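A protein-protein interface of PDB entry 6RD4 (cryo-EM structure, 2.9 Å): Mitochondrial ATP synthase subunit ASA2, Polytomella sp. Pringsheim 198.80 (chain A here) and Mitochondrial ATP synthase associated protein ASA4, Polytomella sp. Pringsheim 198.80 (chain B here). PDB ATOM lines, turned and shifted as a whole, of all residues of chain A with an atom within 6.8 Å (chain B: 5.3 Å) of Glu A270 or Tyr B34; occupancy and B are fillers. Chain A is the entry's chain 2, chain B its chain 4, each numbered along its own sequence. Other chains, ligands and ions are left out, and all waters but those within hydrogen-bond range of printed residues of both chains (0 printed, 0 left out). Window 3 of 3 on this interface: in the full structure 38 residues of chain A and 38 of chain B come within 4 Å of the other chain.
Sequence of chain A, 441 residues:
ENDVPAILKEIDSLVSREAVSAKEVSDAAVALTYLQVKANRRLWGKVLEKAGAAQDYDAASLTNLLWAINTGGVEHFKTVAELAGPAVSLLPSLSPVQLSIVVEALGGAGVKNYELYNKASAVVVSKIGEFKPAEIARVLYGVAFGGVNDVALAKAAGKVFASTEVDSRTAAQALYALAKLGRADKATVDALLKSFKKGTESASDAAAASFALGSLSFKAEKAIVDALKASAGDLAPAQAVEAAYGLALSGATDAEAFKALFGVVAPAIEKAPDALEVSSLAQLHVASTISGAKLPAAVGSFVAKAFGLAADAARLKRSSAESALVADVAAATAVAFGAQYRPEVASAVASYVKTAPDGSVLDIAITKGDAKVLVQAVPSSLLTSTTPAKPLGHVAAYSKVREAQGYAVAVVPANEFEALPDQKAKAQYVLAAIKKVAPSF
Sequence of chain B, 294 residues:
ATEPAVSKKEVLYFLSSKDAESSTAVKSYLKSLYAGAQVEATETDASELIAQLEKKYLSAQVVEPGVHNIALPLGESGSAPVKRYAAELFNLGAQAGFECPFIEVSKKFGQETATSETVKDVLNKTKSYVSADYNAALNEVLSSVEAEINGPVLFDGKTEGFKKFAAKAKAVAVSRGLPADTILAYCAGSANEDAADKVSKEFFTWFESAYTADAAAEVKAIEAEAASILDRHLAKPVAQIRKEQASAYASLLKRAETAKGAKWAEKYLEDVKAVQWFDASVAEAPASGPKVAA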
ATOM      1  N   VAL A 265       9.425  34.132 -12.265  1.00  0.00           N
ATOM      2  CA  VAL A 265      10.550  33.530 -12.955  1.00  0.00           C
ATOM      3  C   VAL A 265      10.146  32.239 -13.640  1.00  0.00           C
ATOM      4  O   VAL A 265      10.781  31.825 -14.608  1.00  0.00           O
ATOM      5  CB  VAL A 265      11.714  33.322 -11.977  1.00  0.00           C
ATOM      6  CG1 VAL A 265      12.151  34.639 -11.443  1.00  0.00           C
ATOM      7  CG2 VAL A 265      11.304  32.459 -10.850  1.00  0.00           C
ATOM      8  N   ALA A 266       9.087  31.586 -13.173  1.00  0.00           N
ATOM      9  CA  ALA A 266       8.690  30.324 -13.799  1.00  0.00           C
ATOM     10  C   ALA A 266       8.076  30.495 -15.187  1.00  0.00           C
ATOM     11  O   ALA A 266       8.476  29.748 -16.094  1.00  0.00           O
ATOM     12  CB  ALA A 266       7.784  29.529 -12.855  1.00  0.00           C
ATOM     13  N   PRO A 267       7.137  31.424 -15.450  1.00  0.00           N
ATOM     14  CA  PRO A 267       6.685  31.570 -16.840  1.00  0.00           C
ATOM     15  C   PRO A 267       7.700  32.252 -17.728  1.00  0.00           C
ATOM     16  O   PRO A 267       7.552  32.206 -18.953  1.00  0.00           O
ATOM     17  CB  PRO A 267       5.413  32.414 -16.718  1.00  0.00           C
ATOM     18  CG  PRO A 267       5.034  32.332 -15.322  1.00  0.00           C
ATOM     19  CD  PRO A 267       6.313  32.299 -14.597  1.00  0.00           C
ATOM     20  N   ALA A 268       8.713  32.899 -17.149  1.00  0.00           N
ATOM     21  CA  ALA A 268       9.773  33.485 -17.953  1.00  0.00           C
ATOM     22  C   ALA A 268      10.734  32.421 -18.456  1.00  0.00           C
ATOM     23  O   ALA A 268      11.143  32.452 -19.620  1.00  0.00           O
ATOM     24  CB  ALA A 268      10.514  34.530 -17.137  1.00  0.00           C
ATOM     25  N   ILE A 269      11.105  31.474 -17.599  1.00  0.00           N
ATOM     26  CA  ILE A 269      11.934  30.355 -18.029  1.00  0.00           C
ATOM     27  C   ILE A 269      11.144  29.421 -18.935  1.00  0.00           C
ATOM     28  O   ILE A 269      11.688  28.846 -19.880  1.00  0.00           O
ATOM     29  CB  ILE A 269      12.500  29.634 -16.792  1.00  0.00           C
ATOM     30  CG1 ILE A 269      13.370  30.591 -15.998  1.00  0.00           C
ATOM     31  CG2 ILE A 269      13.353  28.456 -17.165  1.00  0.00           C
ATOM     32  CD1 ILE A 269      13.711  30.098 -14.647  1.00  0.00           C
ATOM     33  N   GLU A 270       9.840  29.286 -18.699  1.00  0.00           N
ATOM     34  CA  GLU A 270       9.026  28.460 -19.580  1.00  0.00           C
ATOM     35  C   GLU A 270       8.856  29.092 -20.953  1.00  0.00           C
ATOM     36  O   GLU A 270       8.672  28.375 -21.942  1.00  0.00           O
ATOM     37  CB  GLU A 270       7.662  28.202 -18.949  1.00  0.00           C
ATOM     38  CG  GLU A 270       7.699  27.150 -17.872  1.00  0.00           C
ATOM     39  CD  GLU A 270       6.339  26.770 -17.365  1.00  0.00           C
ATOM     40  OE1 GLU A 270       6.268  25.892 -16.484  1.00  0.00           O
ATOM     41  OE2 GLU A 270       5.341  27.339 -17.848  1.00  0.00           O
ATOM     42  N   LYS A 271       8.924  30.417 -21.040  1.00  0.00           N
ATOM     43  CA  LYS A 271       8.746  31.070 -22.330  1.00  0.00           C
ATOM     44  C   LYS A 271      10.039  31.055 -23.128  1.00  0.00           C
ATOM     45  O   LYS A 271      10.039  30.731 -24.319  1.00  0.00           O
ATOM     46  CB  LYS A 271       8.235  32.492 -22.126  1.00  0.00           C
ATOM     47  CG  LYS A 271       7.787  33.191 -23.391  1.00  0.00           C
ATOM     48  CD  LYS A 271       7.226  34.556 -23.048  1.00  0.00           C
ATOM     49  CE  LYS A 271       5.880  34.412 -22.347  1.00  0.00           C
ATOM     50  NZ  LYS A 271       5.220  35.715 -22.073  1.00  0.00           N
ATOM     51  N   ALA A 272      11.149  31.407 -22.489  1.00  0.00           N
ATOM     52  CA  ALA A 272      12.470  31.250 -23.078  1.00  0.00           C
ATOM     53  C   ALA A 272      13.443  30.826 -21.990  1.00  0.00           C
ATOM     54  O   ALA A 272      13.790  31.632 -21.120  1.00  0.00           O
ATOM     55  CB  ALA A 272      12.933  32.540 -23.743  1.00  0.00           C
ATOM     56  N   PRO A 273      13.893  29.571 -21.998  1.00  0.00           N
ATOM     57  CA  PRO A 273      14.766  29.089 -20.917  1.00  0.00           C
ATOM     58  C   PRO A 273      16.155  29.674 -20.955  1.00  0.00           C
ATOM     59  O   PRO A 273      16.828  29.705 -19.920  1.00  0.00           O
ATOM     60  CB  PRO A 273      14.800  27.577 -21.143  1.00  0.00           C
ATOM     61  CG  PRO A 273      13.728  27.301 -22.138  1.00  0.00           C
ATOM     62  CD  PRO A 273      13.580  28.510 -22.960  1.00  0.00           C
ATOM     63  N   ASP A 274      16.596  30.152 -22.106  1.00  0.00           N
ATOM     64  CA  ASP A 274      17.896  30.773 -22.255  1.00  0.00           C
ATOM     65  C   ASP A 274      17.874  32.267 -21.964  1.00  0.00           C
ATOM     66  O   ASP A 274      18.837  32.961 -22.289  1.00  0.00           O
ATOM     67  CB  ASP A 274      18.412  30.514 -23.662  1.00  0.00           C
ATOM     68  CG  ASP A 274      17.368  30.783 -24.711  1.00  0.00           C
ATOM     69  OD1 ASP A 274      16.231  31.116 -24.336  1.00  0.00           O
ATOM     70  OD2 ASP A 274      17.672  30.652 -25.913  1.00  0.00           O
ATOM     71  N   PRO A 296       7.510  24.734 -11.161  1.00  0.00           N
ATOM     72  CA  PRO A 296       6.935  23.830 -12.165  1.00  0.00           C
ATOM     73  C   PRO A 296       7.832  22.648 -12.511  1.00  0.00           C
ATOM     74  O   PRO A 296       9.030  22.629 -12.238  1.00  0.00           O
ATOM     75  CB  PRO A 296       6.733  24.741 -13.374  1.00  0.00           C
ATOM     76  CG  PRO A 296       6.392  26.028 -12.769  1.00  0.00           C
ATOM     77  CD  PRO A 296       7.140  26.128 -11.464  1.00  0.00           C
ATOM     78  N   ALA A 297       7.207  21.632 -13.108  1.00  0.00           N
ATOM     79  CA  ALA A 297       7.885  20.358 -13.303  1.00  0.00           C
ATOM     80  C   ALA A 297       8.946  20.443 -14.382  1.00  0.00           C
ATOM     81  O   ALA A 297       9.930  19.697 -14.342  1.00  0.00           O
ATOM     82  CB  ALA A 297       6.870  19.271 -13.647  1.00  0.00           C
ATOM     83  N   ALA A 298       8.773  21.334 -15.349  1.00  0.00           N
ATOM     84  CA  ALA A 298       9.785  21.528 -16.369  1.00  0.00           C
ATOM     85  C   ALA A 298      10.832  22.544 -15.961  1.00  0.00           C
ATOM     86  O   ALA A 298      11.878  22.612 -16.604  1.00  0.00           O
ATOM     87  CB  ALA A 298       9.140  21.963 -17.687  1.00  0.00           C
ATOM     88  N   VAL A 299      10.587  23.318 -14.912  1.00  0.00           N
ATOM     89  CA  VAL A 299      11.495  24.368 -14.486  1.00  0.00           C
ATOM     90  C   VAL A 299      12.444  23.879 -13.408  1.00  0.00           C
ATOM     91  O   VAL A 299      13.658  24.014 -13.541  1.00  0.00           O
ATOM     92  CB  VAL A 299      10.697  25.604 -14.013  1.00  0.00           C
ATOM     93  CG1 VAL A 299      11.576  26.557 -13.243  1.00  0.00           C
ATOM     94  CG2 VAL A 299      10.108  26.303 -15.185  1.00  0.00           C
ATOM     95  N   PHE A 302      14.918  21.651 -14.587  1.00  0.00           N
ATOM     96  CA  PHE A 302      15.852  22.317 -15.485  1.00  0.00           C
ATOM     97  C   PHE A 302      16.855  23.164 -14.720  1.00  0.00           C
ATOM     98  O   PHE A 302      18.036  23.177 -15.063  1.00  0.00           O
ATOM     99  CB  PHE A 302      15.082  23.163 -16.491  1.00  0.00           C
ATOM    100  CG  PHE A 302      15.905  24.197 -17.182  1.00  0.00           C
ATOM    101  CD1 PHE A 302      15.697  25.537 -16.932  1.00  0.00           C
ATOM    102  CD2 PHE A 302      16.864  23.836 -18.103  1.00  0.00           C
ATOM    103  CE1 PHE A 302      16.441  26.487 -17.564  1.00  0.00           C
ATOM    104  CE2 PHE A 302      17.605  24.795 -18.745  1.00  0.00           C
ATOM    105  CZ  PHE A 302      17.389  26.115 -18.473  1.00  0.00           C
ATOM    106  N   LYS A 305      19.770  21.046 -13.170  1.00  0.00           N
ATOM    107  CA  LYS A 305      20.953  20.807 -13.975  1.00  0.00           C
ATOM    108  C   LYS A 305      21.831  22.042 -14.014  1.00  0.00           C
ATOM    109  O   LYS A 305      23.059  21.936 -14.025  1.00  0.00           O
ATOM    110  CB  LYS A 305      20.553  20.396 -15.384  1.00  0.00           C
ATOM    111  CG  LYS A 305      19.348  19.514 -15.439  1.00  0.00           C
ATOM    112  CD  LYS A 305      19.122  19.018 -16.838  1.00  0.00           C
ATOM    113  CE  LYS A 305      17.788  18.345 -16.958  1.00  0.00           C
ATOM    114  NZ  LYS A 305      17.524  17.966 -18.354  1.00  0.00           N
ATOM    115  N   TYR B  29      22.272  24.906 -26.019  1.00  0.00           N
ATOM    116  CA  TYR B  29      22.507  23.821 -25.077  1.00  0.00           C
ATOM    117  C   TYR B  29      21.546  23.900 -23.907  1.00  0.00           C
ATOM    118  O   TYR B  29      21.031  22.876 -23.458  1.00  0.00           O
ATOM    119  CB  TYR B  29      23.943  23.873 -24.580  1.00  0.00           C
ATOM    120  CG  TYR B  29      24.310  22.832 -23.563  1.00  0.00           C
ATOM    121  CD1 TYR B  29      24.601  21.541 -23.952  1.00  0.00           C
ATOM    122  CD2 TYR B  29      24.404  23.150 -22.218  1.00  0.00           C
ATOM    123  CE1 TYR B  29      24.953  20.595 -23.038  1.00  0.00           C
ATOM    124  CE2 TYR B  29      24.753  22.207 -21.297  1.00  0.00           C
ATOM    125  CZ  TYR B  29      25.025  20.933 -21.713  1.00  0.00           C
ATOM    126  OH  TYR B  29      25.381  19.983 -20.797  1.00  0.00           O
ATOM    127  N   LEU B  30      21.282  25.106 -23.413  1.00  0.00           N
ATOM    128  CA  LEU B  30      20.334  25.277 -22.320  1.00  0.00           C
ATOM    129  C   LEU B  30      18.905  25.044 -22.789  1.00  0.00           C
ATOM    130  O   LEU B  30      18.022  24.772 -21.973  1.00  0.00           O
ATOM    131  CB  LEU B  30      20.471  26.674 -21.718  1.00  0.00           C
ATOM    132  CG  LEU B  30      21.371  26.961 -20.517  1.00  0.00           C
ATOM    133  CD1 LEU B  30      20.871  26.278 -19.298  1.00  0.00           C
ATOM    134  CD2 LEU B  30      22.776  26.518 -20.775  1.00  0.00           C
ATOM    135  N   LYS B  31      18.653  25.166 -24.089  1.00  0.00           N
ATOM    136  CA  LYS B  31      17.346  24.816 -24.623  1.00  0.00           C
ATOM    137  C   LYS B  31      17.193  23.312 -24.773  1.00  0.00           C
ATOM    138  O   LYS B  31      16.072  22.800 -24.747  1.00  0.00           O
ATOM    139  CB  LYS B  31      17.122  25.512 -25.960  1.00  0.00           C
ATOM    140  CG  LYS B  31      16.544  26.907 -25.815  1.00  0.00           C
ATOM    141  CD  LYS B  31      16.669  27.697 -27.098  1.00  0.00           C
ATOM    142  CE  LYS B  31      16.015  26.976 -28.258  1.00  0.00           C
ATOM    143  NZ  LYS B  31      16.161  27.732 -29.525  1.00  0.00           N
ATOM    144  N   SER B  32      18.297  22.593 -24.946  1.00  0.00           N
ATOM    145  CA  SER B  32      18.236  21.139 -24.904  1.00  0.00           C
ATOM    146  C   SER B  32      18.055  20.643 -23.480  1.00  0.00           C
ATOM    147  O   SER B  32      17.387  19.633 -23.249  1.00  0.00           O
ATOM    148  CB  SER B  32      19.498  20.544 -25.511  1.00  0.00           C
ATOM    149  OG  SER B  32      19.479  19.139 -25.401  1.00  0.00           O
ATOM    150  N   LEU B  33      18.648  21.330 -22.512  1.00  0.00           N
ATOM    151  CA  LEU B  33      18.466  20.938 -21.126  1.00  0.00           C
ATOM    152  C   LEU B  33      17.117  21.356 -20.577  1.00  0.00           C
ATOM    153  O   LEU B  33      16.753  20.930 -19.480  1.00  0.00           O
ATOM    154  CB  LEU B  33      19.555  21.526 -20.240  1.00  0.00           C
ATOM    155  CG  LEU B  33      20.997  21.061 -20.357  1.00  0.00           C
ATOM    156  CD1 LEU B  33      21.615  21.213 -19.008  1.00  0.00           C
ATOM    157  CD2 LEU B  33      21.093  19.649 -20.828  1.00  0.00           C
ATOM    158  N   TYR B  34      16.382  22.214 -21.273  1.00  0.00           N
ATOM    159  CA  TYR B  34      15.004  22.437 -20.863  1.00  0.00           C
ATOM    160  C   TYR B  34      14.109  21.309 -21.321  1.00  0.00           C
ATOM    161  O   TYR B  34      13.150  20.962 -20.631  1.00  0.00           O
ATOM    162  CB  TYR B  34      14.478  23.756 -21.401  1.00  0.00           C
ATOM    163  CG  TYR B  34      13.110  24.063 -20.880  1.00  0.00           C
ATOM    164  CD1 TYR B  34      12.006  23.991 -21.705  1.00  0.00           C
ATOM    165  CD2 TYR B  34      12.921  24.400 -19.553  1.00  0.00           C
ATOM    166  CE1 TYR B  34      10.760  24.260 -21.232  1.00  0.00           C
ATOM    167  CE2 TYR B  34      11.677  24.674 -19.070  1.00  0.00           C
ATOM    168  CZ  TYR B  34      10.601  24.599 -19.915  1.00  0.00           C
ATOM    169  OH  TYR B  34       9.346  24.862 -19.445  1.00  0.00           O
ATOM    170  N   ALA B  35      14.420  20.710 -22.462  1.00  0.00           N
ATOM    171  CA  ALA B  35      13.688  19.547 -22.944  1.00  0.00           C
ATOM    172  C   ALA B  35      14.311  18.253 -22.431  1.00  0.00           C
ATOM    173  O   ALA B  35      14.550  17.307 -23.178  1.00  0.00           O
ATOM    174  CB  ALA B  35      13.633  19.567 -24.464  1.00  0.00           C
ATOM    175  N   GLY B  36      14.584  18.228 -21.126  1.00  0.00           N
ATOM    176  CA  GLY B  36      14.856  17.024 -20.374  1.00  0.00           C
ATOM    177  C   GLY B  36      16.099  16.245 -20.728  1.00  0.00           C
ATOM    178  O   GLY B  36      16.229  15.104 -20.276  1.00  0.00           O
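O of Leu B33 is in hydrogen-bond range of NZ of Lys A305 (3.3 Å).
Among the printed residues, merely in contact across the chains: Phe A302 with Leu B33, Ala A298 with Tyr B34, Glu A270 with Tyr B34, Phe A302 with Leu B30, Lys A305 with Gly B36, Asp A274 with Lys B31, Pro A273 with Tyr B34 and Phe A302 with Tyr B34.
Ala A268 touches none of the printed residues of chain B.
Of chain B, only Tyr B34 comes within 4 Å of Glu A270.
Printed residues of chain B within 4 Å of Phe A302: Leu B30, Leu B33 and Tyr B34.
Of the printed residues of chain B, Lys A305 touches Leu B33 (3.3 Å) and Gly B36 (3.3 Å).
Of the printed residues of chain A, Lys B31 touches Asp A274 (3.3 Å).
Ala B35 touches none of the printed residues of chain A.
Printed residues of chain A within 4 Å of Gly B36: Lys A305.
Of the 8 printed residues of chain B, 5 touch a printed residue of chain A.
Hydrophobic or aromatic side chains of chain B that line the printed part of chain A: Leu B30, Leu B33 and Tyr B34.
Printed residues of chain A that touch a printed residue of chain B: Glu A270, Pro A273, Asp A274, Ala A298, Phe A302 and Lys A305.
Hydrophobic or aromatic side chains of chain A within 4 Å of the printed part of chain B: Pro A273, Ala A298 and Phe A302.
Among the printed residues, no Asp or Glu carboxylate lies within 4 Å of a Lys or Arg side-chain nitrogen of the other chain.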
